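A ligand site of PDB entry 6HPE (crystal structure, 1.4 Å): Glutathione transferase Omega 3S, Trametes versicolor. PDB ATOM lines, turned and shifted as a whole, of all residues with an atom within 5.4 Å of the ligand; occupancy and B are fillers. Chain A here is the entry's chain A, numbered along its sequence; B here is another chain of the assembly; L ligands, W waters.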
ATOM      1  N   PHE A  14     -15.299 -27.865  -6.593  1.00  0.00           N
ATOM      2  CA  PHE A  14     -14.565 -27.288  -7.699  1.00  0.00           C
ATOM      3  C   PHE A  14     -15.390 -26.241  -8.464  1.00  0.00           C
ATOM      4  O   PHE A  14     -14.803 -25.433  -9.171  1.00  0.00           O
ATOM      5  CB  PHE A  14     -14.104 -28.354  -8.691  1.00  0.00           C
ATOM      6  CG  PHE A  14     -15.207 -28.938  -9.496  1.00  0.00           C
ATOM      7  CD1 PHE A  14     -15.610 -28.349 -10.685  1.00  0.00           C
ATOM      8  CD2 PHE A  14     -15.850 -30.062  -9.067  1.00  0.00           C
ATOM      9  CE1 PHE A  14     -16.654 -28.907 -11.426  1.00  0.00           C
ATOM     10  CE2 PHE A  14     -16.892 -30.605  -9.817  1.00  0.00           C
ATOM     11  CZ  PHE A  14     -17.286 -29.989 -10.983  1.00  0.00           C
ATOM     12  N   SER A  15     -16.733 -26.296  -8.376  1.00  0.00           N
ATOM     13  CA  SER A  15     -17.577 -25.617  -9.354  1.00  0.00           C
ATOM     14  C   SER A  15     -17.702 -24.123  -9.053  1.00  0.00           C
ATOM     15  O   SER A  15     -18.294 -23.768  -8.024  1.00  0.00           O
ATOM     16  CB  SER A  15     -18.991 -26.243  -9.354  1.00  0.00           C
ATOM     17  OG  SER A  15     -19.879 -25.431 -10.111  1.00  0.00           O
ATOM     18  N   PRO A  16     -17.221 -23.233  -9.921  1.00  0.00           N
ATOM     19  CA  PRO A  16     -17.397 -21.809  -9.654  1.00  0.00           C
ATOM     20  C   PRO A  16     -18.856 -21.393  -9.733  1.00  0.00           C
ATOM     21  O   PRO A  16     -19.273 -20.463  -9.065  1.00  0.00           O
ATOM     22  CB  PRO A  16     -16.553 -21.146 -10.734  1.00  0.00           C
ATOM     23  CG  PRO A  16     -16.553 -22.158 -11.877  1.00  0.00           C
ATOM     24  CD  PRO A  16     -16.491 -23.470 -11.183  1.00  0.00           C
ATOM     25  N   TYR A  17     -19.653 -22.076 -10.583  1.00  0.00           N
ATOM     26  CA  TYR A  17     -21.070 -21.751 -10.689  1.00  0.00           C
ATOM     27  C   TYR A  17     -21.796 -22.045  -9.386  1.00  0.00           C
ATOM     28  O   TYR A  17     -22.645 -21.276  -8.963  1.00  0.00           O
ATOM     29  CB  TYR A  17     -21.702 -22.546 -11.857  1.00  0.00           C
ATOM     30  CG  TYR A  17     -21.107 -22.189 -13.194  1.00  0.00           C
ATOM     31  CD1 TYR A  17     -21.565 -21.061 -13.882  1.00  0.00           C
ATOM     32  CD2 TYR A  17     -20.115 -22.965 -13.752  1.00  0.00           C
ATOM     33  CE1 TYR A  17     -21.021 -20.723 -15.107  1.00  0.00           C
ATOM     34  CE2 TYR A  17     -19.571 -22.641 -14.978  1.00  0.00           C
ATOM     35  CZ  TYR A  17     -20.060 -21.542 -15.653  1.00  0.00           C
ATOM     36  OH  TYR A  17     -19.460 -21.309 -16.902  1.00  0.00           O
ATOM     37  N   ARG A  20     -20.892 -19.412  -6.681  1.00  0.00           N
ATOM     38  CA  ARG A  20     -21.677 -18.184  -6.747  1.00  0.00           C
ATOM     39  C   ARG A  20     -22.830 -18.205  -5.773  1.00  0.00           C
ATOM     40  O   ARG A  20     -23.115 -17.210  -5.086  1.00  0.00           O
ATOM     41  CB  ARG A  20     -22.332 -18.010  -8.136  1.00  0.00           C
ATOM     42  CG  ARG A  20     -21.426 -17.830  -9.325  1.00  0.00           C
ATOM     43  CD  ARG A  20     -22.232 -17.767 -10.637  1.00  0.00           C
ATOM     44  NE  ARG A  20     -21.458 -17.079 -11.659  1.00  0.00           N
ATOM     45  CZ  ARG A  20     -21.765 -16.995 -12.941  1.00  0.00           C
ATOM     46  NH1 ARG A  20     -22.771 -17.693 -13.466  1.00  0.00           N
ATOM     47  NH2 ARG A  20     -20.996 -16.273 -13.728  1.00  0.00           N
ATOM     48  N   VAL A  37     -22.095 -33.348  -4.709  1.00  0.00           N
ATOM     49  CA  VAL A  37     -22.119 -34.513  -5.577  1.00  0.00           C
ATOM     50  C   VAL A  37     -20.696 -34.966  -5.853  1.00  0.00           C
ATOM     51  O   VAL A  37     -19.717 -34.228  -5.628  1.00  0.00           O
ATOM     52  CB  VAL A  37     -22.898 -34.231  -6.854  1.00  0.00           C
ATOM     53  CG1 VAL A  37     -24.326 -33.759  -6.517  1.00  0.00           C
ATOM     54  CG2 VAL A  37     -22.095 -33.202  -7.714  1.00  0.00           C
ATOM     55  N   ASP A  38     -20.584 -36.182  -6.390  1.00  0.00           N
ATOM     56  CA  ASP A  38     -19.309 -36.829  -6.673  1.00  0.00           C
ATOM     57  C   ASP A  38     -19.277 -37.134  -8.158  1.00  0.00           C
ATOM     58  O   ASP A  38     -19.852 -38.132  -8.620  1.00  0.00           O
ATOM     59  CB  ASP A  38     -19.159 -38.097  -5.807  1.00  0.00           C
ATOM     60  CG  ASP A  38     -17.886 -38.877  -6.115  1.00  0.00           C
ATOM     61  OD1 ASP A  38     -17.029 -38.380  -6.894  1.00  0.00           O
ATOM     62  OD2 ASP A  38     -17.755 -40.005  -5.594  1.00  0.00           O
ATOM     63  N   ILE A  39     -18.638 -36.259  -8.945  1.00  0.00           N
ATOM     64  CA  ILE A  39     -18.686 -36.397 -10.399  1.00  0.00           C
ATOM     65  C   ILE A  39     -17.816 -37.531 -10.904  1.00  0.00           C
ATOM     66  O   ILE A  39     -17.868 -37.848 -12.111  1.00  0.00           O
ATOM     67  CB  ILE A  39     -18.264 -35.083 -11.098  1.00  0.00           C
ATOM     68  CG1 ILE A  39     -16.825 -34.731 -10.736  1.00  0.00           C
ATOM     69  CG2 ILE A  39     -19.257 -33.933 -10.698  1.00  0.00           C
ATOM     70  CD1 ILE A  39     -16.176 -33.757 -11.690  1.00  0.00           C
ATOM     71  N   ARG A  41     -18.072 -40.593  -9.752  1.00  0.00           N
ATOM     72  CA  ARG A  41     -18.908 -41.776  -9.732  1.00  0.00           C
ATOM     73  C   ARG A  41     -20.173 -41.507 -10.524  1.00  0.00           C
ATOM     74  O   ARG A  41     -20.444 -40.377 -10.961  1.00  0.00           O
ATOM     75  CB  ARG A  41     -19.181 -42.237  -8.305  1.00  0.00           C
ATOM     76  CG  ARG A  41     -17.972 -42.952  -7.716  1.00  0.00           C
ATOM     77  CD  ARG A  41     -18.300 -43.678  -6.433  1.00  0.00           C
ATOM     78  NE  ARG A  41     -18.813 -42.761  -5.426  1.00  0.00           N
ATOM     79  CZ  ARG A  41     -19.943 -42.906  -4.739  1.00  0.00           C
ATOM     80  NH1 ARG A  41     -20.719 -43.974  -4.916  1.00  0.00           N
ATOM     81  NH2 ARG A  41     -20.297 -41.990  -3.844  1.00  0.00           N
ATOM     82  N   ASN A  42     -20.921 -42.573 -10.767  1.00  0.00           N
ATOM     83  CA  ASN A  42     -22.067 -42.454 -11.644  1.00  0.00           C
ATOM     84  C   ASN A  42     -23.042 -41.445 -11.073  1.00  0.00           C
ATOM     85  O   ASN A  42     -23.193 -41.330  -9.853  1.00  0.00           O
ATOM     86  CB  ASN A  42     -22.737 -43.818 -11.832  1.00  0.00           C
ATOM     87  CG  ASN A  42     -21.775 -44.841 -12.407  1.00  0.00           C
ATOM     88  OD1 ASN A  42     -21.317 -44.706 -13.555  1.00  0.00           O
ATOM     89  ND2 ASN A  42     -21.447 -45.855 -11.617  1.00  0.00           N
ATOM     90  N   MET A  43     -23.677 -40.681 -11.944  1.00  0.00           N
ATOM     91  CA  MET A  43     -24.673 -39.739 -11.481  1.00  0.00           C
ATOM     92  C   MET A  43     -25.848 -40.517 -10.900  1.00  0.00           C
ATOM     93  O   MET A  43     -26.384 -41.422 -11.564  1.00  0.00           O
ATOM     94  CB  MET A  43     -25.158 -38.836 -12.603  1.00  0.00           C
ATOM     95  CG  MET A  43     -26.278 -37.900 -12.206  1.00  0.00           C
ATOM     96  SD  MET A  43     -26.968 -37.087 -13.668  1.00  0.00           S
ATOM     97  CE  MET A  43     -27.807 -38.483 -14.412  1.00  0.00           C
ATOM     98  N   PRO A  44     -26.307 -40.173  -9.702  1.00  0.00           N
ATOM     99  CA  PRO A  44     -27.444 -40.881  -9.100  1.00  0.00           C
ATOM    100  C   PRO A  44     -28.684 -40.729  -9.973  1.00  0.00           C
ATOM    101  O   PRO A  44     -28.891 -39.697 -10.616  1.00  0.00           O
ATOM    102  CB  PRO A  44     -27.620 -40.169  -7.749  1.00  0.00           C
ATOM    103  CG  PRO A  44     -26.398 -39.399  -7.515  1.00  0.00           C
ATOM    104  CD  PRO A  44     -25.771 -39.120  -8.828  1.00  0.00           C
ATOM    105  N   PHE A  47     -30.800 -37.551  -9.654  1.00  0.00           N
ATOM    106  CA  PHE A  47     -30.295 -36.203  -9.866  1.00  0.00           C
ATOM    107  C   PHE A  47     -31.072 -35.524 -10.993  1.00  0.00           C
ATOM    108  O   PHE A  47     -31.426 -34.346 -10.873  1.00  0.00           O
ATOM    109  CB  PHE A  47     -28.780 -36.140 -10.092  1.00  0.00           C
ATOM    110  CG  PHE A  47     -28.274 -34.741 -10.170  1.00  0.00           C
ATOM    111  CD1 PHE A  47     -28.022 -34.044  -9.010  1.00  0.00           C
ATOM    112  CD2 PHE A  47     -28.141 -34.128 -11.374  1.00  0.00           C
ATOM    113  CE1 PHE A  47     -27.624 -32.739  -9.082  1.00  0.00           C
ATOM    114  CE2 PHE A  47     -27.720 -32.816 -11.451  1.00  0.00           C
ATOM    115  CZ  PHE A  47     -27.446 -32.139 -10.297  1.00  0.00           C
ATOM    116  N   LYS A  54     -28.238 -32.064 -16.157  1.00  0.00           N
ATOM    117  CA  LYS A  54     -27.078 -32.682 -15.542  1.00  0.00           C
ATOM    118  C   LYS A  54     -26.072 -31.617 -15.146  1.00  0.00           C
ATOM    119  O   LYS A  54     -24.862 -31.758 -15.349  1.00  0.00           O
ATOM    120  CB  LYS A  54     -26.433 -33.720 -16.446  1.00  0.00           C
ATOM    121  CG  LYS A  54     -27.436 -34.769 -16.861  1.00  0.00           C
ATOM    122  CD  LYS A  54     -26.828 -35.948 -17.604  1.00  0.00           C
ATOM    123  CE  LYS A  54     -25.928 -35.556 -18.777  1.00  0.00           C
ATOM    124  NZ  LYS A  54     -26.646 -35.648 -20.087  1.00  0.00           N
ATOM    125  N   LYS A  55     -26.600 -30.484 -14.654  1.00  0.00           N
ATOM    126  CA  LYS A  55     -25.734 -29.387 -14.243  1.00  0.00           C
ATOM    127  C   LYS A  55     -25.757 -29.210 -12.730  1.00  0.00           C
ATOM    128  O   LYS A  55     -26.792 -29.379 -12.086  1.00  0.00           O
ATOM    129  CB  LYS A  55     -26.156 -28.063 -14.835  1.00  0.00           C
ATOM    130  CG  LYS A  55     -26.201 -27.980 -16.351  1.00  0.00           C
ATOM    131  CD  LYS A  55     -24.901 -28.012 -16.971  1.00  0.00           C
ATOM    132  CE  LYS A  55     -25.138 -27.952 -18.495  1.00  0.00           C
ATOM    133  NZ  LYS A  55     -23.899 -27.918 -19.216  1.00  0.00           N
ATOM    134  N   ILE A  56     -24.607 -28.741 -12.227  1.00  0.00           N
ATOM    135  CA  ILE A  56     -24.458 -28.201 -10.870  1.00  0.00           C
ATOM    136  C   ILE A  56     -24.222 -26.690 -11.047  1.00  0.00           C
ATOM    137  O   ILE A  56     -23.444 -26.284 -11.896  1.00  0.00           O
ATOM    138  CB  ILE A  56     -23.233 -28.904 -10.215  1.00  0.00           C
ATOM    139  CG1 ILE A  56     -23.641 -30.327  -9.834  1.00  0.00           C
ATOM    140  CG2 ILE A  56     -22.660 -28.109  -9.048  1.00  0.00           C
ATOM    141  CD1 ILE A  56     -24.623 -30.368  -8.817  1.00  0.00           C
ATOM    142  N   PRO A  57     -24.807 -25.832 -10.221  1.00  0.00           N
ATOM    143  CA  PRO A  57     -25.685 -26.137  -9.092  1.00  0.00           C
ATOM    144  C   PRO A  57     -27.083 -26.506  -9.548  1.00  0.00           C
ATOM    145  O   PRO A  57     -27.542 -26.155 -10.626  1.00  0.00           O
ATOM    146  CB  PRO A  57     -25.716 -24.814  -8.320  1.00  0.00           C
ATOM    147  CG  PRO A  57     -25.445 -23.757  -9.407  1.00  0.00           C
ATOM    148  CD  PRO A  57     -24.498 -24.393 -10.325  1.00  0.00           C
ATOM    149  N   GLU A  80     -29.917 -22.914 -13.090  1.00  0.00           N
ATOM    150  CA  GLU A  80     -29.017 -21.869 -13.572  1.00  0.00           C
ATOM    151  C   GLU A  80     -28.595 -20.905 -12.449  1.00  0.00           C
ATOM    152  O   GLU A  80     -29.425 -20.213 -11.831  1.00  0.00           O
ATOM    153  CB  GLU A  80     -29.594 -21.099 -14.768  1.00  0.00           C
ATOM    154  CG  GLU A  80     -29.821 -22.026 -16.004  1.00  0.00           C
ATOM    155  CD  GLU A  80     -28.534 -22.557 -16.535  1.00  0.00           C
ATOM    156  OE1 GLU A  80     -27.682 -21.706 -16.943  1.00  0.00           O
ATOM    157  OE2 GLU A  80     -28.261 -23.784 -16.540  1.00  0.00           O
ATOM    158  N   SER A  81     -27.271 -20.853 -12.255  1.00  0.00           N
ATOM    159  CA  SER A  81     -26.694 -20.092 -11.140  1.00  0.00           C
ATOM    160  C   SER A  81     -27.139 -18.621 -11.118  1.00  0.00           C
ATOM    161  O   SER A  81     -27.431 -18.072 -10.042  1.00  0.00           O
ATOM    162  CB  SER A  81     -25.191 -20.192 -11.151  1.00  0.00           C
ATOM    163  OG  SER A  81     -24.589 -19.609 -12.283  1.00  0.00           O
ATOM    164  N   LEU A  82     -27.163 -17.929 -12.258  1.00  0.00           N
ATOM    165  CA  LEU A  82     -27.536 -16.516 -12.163  1.00  0.00           C
ATOM    166  C   LEU A  82     -29.017 -16.336 -11.797  1.00  0.00           C
ATOM    167  O   LEU A  82     -29.389 -15.348 -11.138  1.00  0.00           O
ATOM    168  CB  LEU A  82     -27.209 -15.748 -13.444  1.00  0.00           C
ATOM    169  CG  LEU A  82     -25.718 -15.611 -13.764  1.00  0.00           C
ATOM    170  CD1 LEU A  82     -25.576 -14.616 -14.961  1.00  0.00           C
ATOM    171  CD2 LEU A  82     -24.868 -15.194 -12.588  1.00  0.00           C
ATOM    172  N   GLU A 116     -20.481 -12.873 -18.141  1.00  0.00           N
ATOM    173  CA  GLU A 116     -21.028 -14.024 -18.848  1.00  0.00           C
ATOM    174  C   GLU A 116     -20.793 -14.037 -20.312  1.00  0.00           C
ATOM    175  O   GLU A 116     -20.519 -15.086 -20.912  1.00  0.00           O
ATOM    176  CB  GLU A 116     -22.516 -14.226 -18.499  1.00  0.00           C
ATOM    177  CG  GLU A 116     -22.938 -15.695 -18.224  1.00  0.00           C
ATOM    178  CD  GLU A 116     -22.501 -16.239 -16.884  1.00  0.00           C
ATOM    179  OE1 GLU A 116     -21.476 -15.774 -16.334  1.00  0.00           O
ATOM    180  OE2 GLU A 116     -23.185 -17.147 -16.373  1.00  0.00           O
ATOM    181  N   ARG A 124     -13.077 -20.388 -20.389  1.00  0.00           N
ATOM    182  CA  ARG A 124     -13.346 -21.740 -20.885  1.00  0.00           C
ATOM    183  C   ARG A 124     -12.412 -22.113 -22.041  1.00  0.00           C
ATOM    184  O   ARG A 124     -11.820 -23.200 -22.028  1.00  0.00           O
ATOM    185  CB  ARG A 124     -14.804 -21.793 -21.310  1.00  0.00           C
ATOM    186  CG  ARG A 124     -15.761 -21.816 -20.165  1.00  0.00           C
ATOM    187  CD  ARG A 124     -17.252 -21.530 -20.583  1.00  0.00           C
ATOM    188  NE  ARG A 124     -17.429 -21.500 -22.046  1.00  0.00           N
ATOM    189  CZ  ARG A 124     -18.217 -20.661 -22.730  1.00  0.00           C
ATOM    190  NH1 ARG A 124     -18.951 -19.705 -22.134  1.00  0.00           N
ATOM    191  NH2 ARG A 124     -18.238 -20.767 -24.065  1.00  0.00           N
ATOM    192  N   PHE A 128      -9.838 -24.931 -20.959  1.00  0.00           N
ATOM    193  CA  PHE A 128     -10.283 -26.253 -21.407  1.00  0.00           C
ATOM    194  C   PHE A 128      -9.821 -26.597 -22.798  1.00  0.00           C
ATOM    195  O   PHE A 128      -9.879 -27.773 -23.174  1.00  0.00           O
ATOM    196  CB  PHE A 128     -11.808 -26.350 -21.419  1.00  0.00           C
ATOM    197  CG  PHE A 128     -12.400 -26.247 -20.083  1.00  0.00           C
ATOM    198  CD1 PHE A 128     -11.912 -27.005 -19.058  1.00  0.00           C
ATOM    199  CD2 PHE A 128     -13.427 -25.369 -19.824  1.00  0.00           C
ATOM    200  CE1 PHE A 128     -12.433 -26.913 -17.790  1.00  0.00           C
ATOM    201  CE2 PHE A 128     -13.962 -25.276 -18.559  1.00  0.00           C
ATOM    202  CZ  PHE A 128     -13.451 -26.041 -17.539  1.00  0.00           C
ATOM    203  N   PHE A 168     -14.768 -17.177 -10.238  1.00  0.00           N
ATOM    204  CA  PHE A 168     -13.896 -17.381 -11.379  1.00  0.00           C
ATOM    205  C   PHE A 168     -12.574 -16.663 -11.209  1.00  0.00           C
ATOM    206  O   PHE A 168     -11.504 -17.251 -11.449  1.00  0.00           O
ATOM    207  CB  PHE A 168     -14.644 -16.937 -12.643  1.00  0.00           C
ATOM    208  CG  PHE A 168     -15.842 -17.776 -12.916  1.00  0.00           C
ATOM    209  CD1 PHE A 168     -17.062 -17.443 -12.349  1.00  0.00           C
ATOM    210  CD2 PHE A 168     -15.750 -18.898 -13.718  1.00  0.00           C
ATOM    211  CE1 PHE A 168     -18.201 -18.247 -12.598  1.00  0.00           C
ATOM    212  CE2 PHE A 168     -16.868 -19.686 -14.003  1.00  0.00           C
ATOM    213  CZ  PHE A 168     -18.070 -19.375 -13.414  1.00  0.00           C
ATOM    214  N   ASN B 117     -27.594 -19.402 -22.383  1.00  0.00           N
ATOM    215  CA  ASN B 117     -26.458 -20.295 -22.173  1.00  0.00           C
ATOM    216  C   ASN B 117     -26.444 -21.477 -23.126  1.00  0.00           C
ATOM    217  O   ASN B 117     -25.349 -21.964 -23.418  1.00  0.00           O
ATOM    218  CB  ASN B 117     -26.423 -20.801 -20.737  1.00  0.00           C
ATOM    219  CG  ASN B 117     -26.023 -19.703 -19.797  1.00  0.00           C
ATOM    220  OD1 ASN B 117     -25.153 -18.896 -20.152  1.00  0.00           O
ATOM    221  ND2 ASN B 117     -26.590 -19.658 -18.622  1.00  0.00           N
ATOM    222  N   TYR B 118     -27.600 -21.976 -23.591  1.00  0.00           N
ATOM    223  CA  TYR B 118     -27.650 -23.208 -24.365  1.00  0.00           C
ATOM    224  C   TYR B 118     -28.245 -23.060 -25.763  1.00  0.00           C
ATOM    225  O   TYR B 118     -27.948 -23.929 -26.627  1.00  0.00           O
ATOM    226  CB  TYR B 118     -28.390 -24.318 -23.598  1.00  0.00           C
ATOM    227  CG  TYR B 118     -27.919 -24.432 -22.192  1.00  0.00           C
ATOM    228  CD1 TYR B 118     -26.604 -24.794 -21.935  1.00  0.00           C
ATOM    229  CD2 TYR B 118     -28.740 -24.160 -21.131  1.00  0.00           C
ATOM    230  CE1 TYR B 118     -26.112 -24.855 -20.605  1.00  0.00           C
ATOM    231  CE2 TYR B 118     -28.284 -24.244 -19.798  1.00  0.00           C
ATOM    232  CZ  TYR B 118     -26.968 -24.583 -19.580  1.00  0.00           C
ATOM    233  OH  TYR B 118     -26.452 -24.657 -18.297  1.00  0.00           O
HETATM  234  O1  LIG L   1     -24.842 -21.041 -14.626  1.00  0.00           O
HETATM  235  C1  LIG L   1     -25.031 -22.273 -14.519  1.00  0.00           C
HETATM  236  O2  LIG L   1     -25.474 -22.780 -13.465  1.00  0.00           O
HETATM  237  C2  LIG L   1     -24.785 -23.114 -15.780  1.00  0.00           C
HETATM  238  N1  LIG L   1     -24.979 -22.253 -16.947  1.00  0.00           N
HETATM  239  C3  LIG L   1     -23.412 -23.699 -15.765  1.00  0.00           C
HETATM  240  C4  LIG L   1     -23.191 -24.781 -14.724  1.00  0.00           C
HETATM  241  C5  LIG L   1     -21.907 -25.613 -14.971  1.00  0.00           C
HETATM  242  O3  LIG L   1     -21.260 -25.606 -15.975  1.00  0.00           O
HETATM  243  N2  LIG L   1     -21.539 -26.391 -13.848  1.00  0.00           N
HETATM  244  C6  LIG L   1     -20.413 -27.287 -13.772  1.00  0.00           C
HETATM  245  C7  LIG L   1     -19.061 -26.574 -13.647  1.00  0.00           C
HETATM  246  O4  LIG L   1     -18.827 -25.912 -12.686  1.00  0.00           O
HETATM  247  N3  LIG L   1     -18.023 -26.825 -14.604  1.00  0.00           N
HETATM  248  C8  LIG L   1     -16.708 -26.230 -14.359  1.00  0.00           C
HETATM  249  C9  LIG L   1     -16.448 -25.019 -15.217  1.00  0.00           C
HETATM  250  O5  LIG L   1     -15.537 -24.233 -14.800  1.00  0.00           O
HETATM  251  O6  LIG L   1     -17.095 -24.828 -16.287  1.00  0.00           O
HETATM  252  C10 LIG L   1     -20.442 -28.299 -14.911  1.00  0.00           C
HETATM  253  S1  LIG L   1     -21.948 -29.328 -14.793  1.00  0.00           S
HETATM  254  C11 LIG L   1     -21.543 -30.646 -13.613  1.00  0.00           C
HETATM  255  S2  LIG L   1     -20.166 -30.638 -12.777  1.00  0.00           S
HETATM  256  N4  LIG L   1     -22.486 -31.699 -13.527  1.00  0.00           N
HETATM  257  C12 LIG L   1     -22.402 -32.739 -12.522  1.00  0.00           C
HETATM  258  C13 LIG L   1     -23.614 -33.652 -12.728  1.00  0.00           C
HETATM  259  C14 LIG L   1     -23.569 -34.723 -11.671  1.00  0.00           C
HETATM  260  C15 LIG L   1     -24.409 -34.680 -10.571  1.00  0.00           C
HETATM  261  C16 LIG L   1     -24.325 -35.669  -9.604  1.00  0.00           C
HETATM  262  C17 LIG L   1     -23.401 -36.688  -9.737  1.00  0.00           C
HETATM  263  C18 LIG L   1     -22.575 -36.732 -10.840  1.00  0.00           C
HETATM  264  C19 LIG L   1     -22.643 -35.742 -11.813  1.00  0.00           C
HETATM  265  O   HOH W   1     -14.190 -22.269 -15.401  1.00  0.00           O
HETATM  266  O   HOH W   2     -17.177 -22.588 -17.580  1.00  0.00           O
HETATM  267  O   HOH W   3     -27.384 -24.725 -12.863  1.00  0.00           O
HETATM  268  O   HOH W   4     -22.349 -25.619 -18.825  1.00  0.00           O
HETATM  269  O   HOH W   5     -23.303 -19.779 -17.595  1.00  0.00           O
HETATM  270  O   HOH W   6     -26.790 -18.963 -14.909  1.00  0.00           O
HETATM  271  O   HOH W   7     -17.267 -28.811 -16.595  1.00  0.00           O
HETATM  272  O   HOH W   8     -23.352 -23.087 -19.279  1.00  0.00           O
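OG of Ser 15 is in hydrogen-bond range of O4 of the ligand, 2.8 Å away. N of Ile 56 sits close to S1 of the ligand (3.7 Å). N of Ser 81 sits at hydrogen-bond distance from O2 of the ligand (2.9 Å). OE1 of Glu 80 is in salt-bridge range of N1 of the ligand (2.8 Å). The side-chain hydroxyl (OH) of Tyr 118 of chain B is in hydrogen-bond range of a nitrogen (N1) of the ligand. The side-chain hydroxyl of Ser 81 is in hydrogen-bond range of an oxygen (O1) of the ligand (2.8 Å). The side-chain amide nitrogen (ND2) of Asn 117 of chain B sits close to a nitrogen (N1) of the ligand (3.5 Å). O of Ile 56 lies within hydrogen-bond range of N2 of the ligand. N4 of the ligand is in hydrogen-bond range of O of Lys 54 (3.0 Å).
Merely in contact with the ligand: Phe 14, Pro 16, Tyr 17, Val 37, Asp 38, Ile 39, Met 43, Pro 44, Phe 47, Lys 55, Pro 57 and Phe 128. Hydrophobic or aromatic side chains that line the ligand: Phe 14, Pro 16, Tyr 17, Val 37, Ile 39, Met 43, Pro 44, Phe 47, Ile 56, Pro 57 and Phe 128. Of the 26 residues printed, 19 come within 4 Å of the ligand.
The side-chain carboxylate (OD2) of Asp 38 lies within salt-bridge range of the guanidinium group (NE) of Arg 41 (3.0 Å). OG of Ser 81 sits at hydrogen-bond distance from NH1 of Arg 20 (2.9 Å). The side-chain amide nitrogen of Asn 117 of chain B sits at hydrogen-bond distance from the side-chain carboxylate of Glu 80 (2.9 Å). The side-chain hydroxyl of Tyr 118 of chain B lies within hydrogen-bond range of the side-chain carboxylate of Glu 80, at 2.7 Å. OG of Ser 15 sits close to N of Tyr 17.
Water W2 lies within hydrogen-bond range of O6 of the ligand (2.6 Å) and OH of Tyr 17 (2.7 Å). Water W3 lies within hydrogen-bond range of the backbone carbonyl oxygen (O) of Pro 57 (2.7 Å), an oxygen (O2) of the ligand (2.8 Å) and the backbone NH (N) of Glu 80 (3.1 Å). Water W6 lies within hydrogen-bond range of O1 of the ligand (2.9 Å), N of Leu 82 (2.9 Å) and N of Ser 81 (3.3 Å). Water W4 bridges the side-chain amino group of Lys 55 and an oxygen (O3) of the ligand. Water W5 lies within hydrogen-bond range of the side-chain carboxylate of Glu 116 (2.9 Å), a nitrogen (N1) of the ligand (3.1 Å) and the side-chain amide oxygen of Asn 117 of chain B (3.3 Å).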
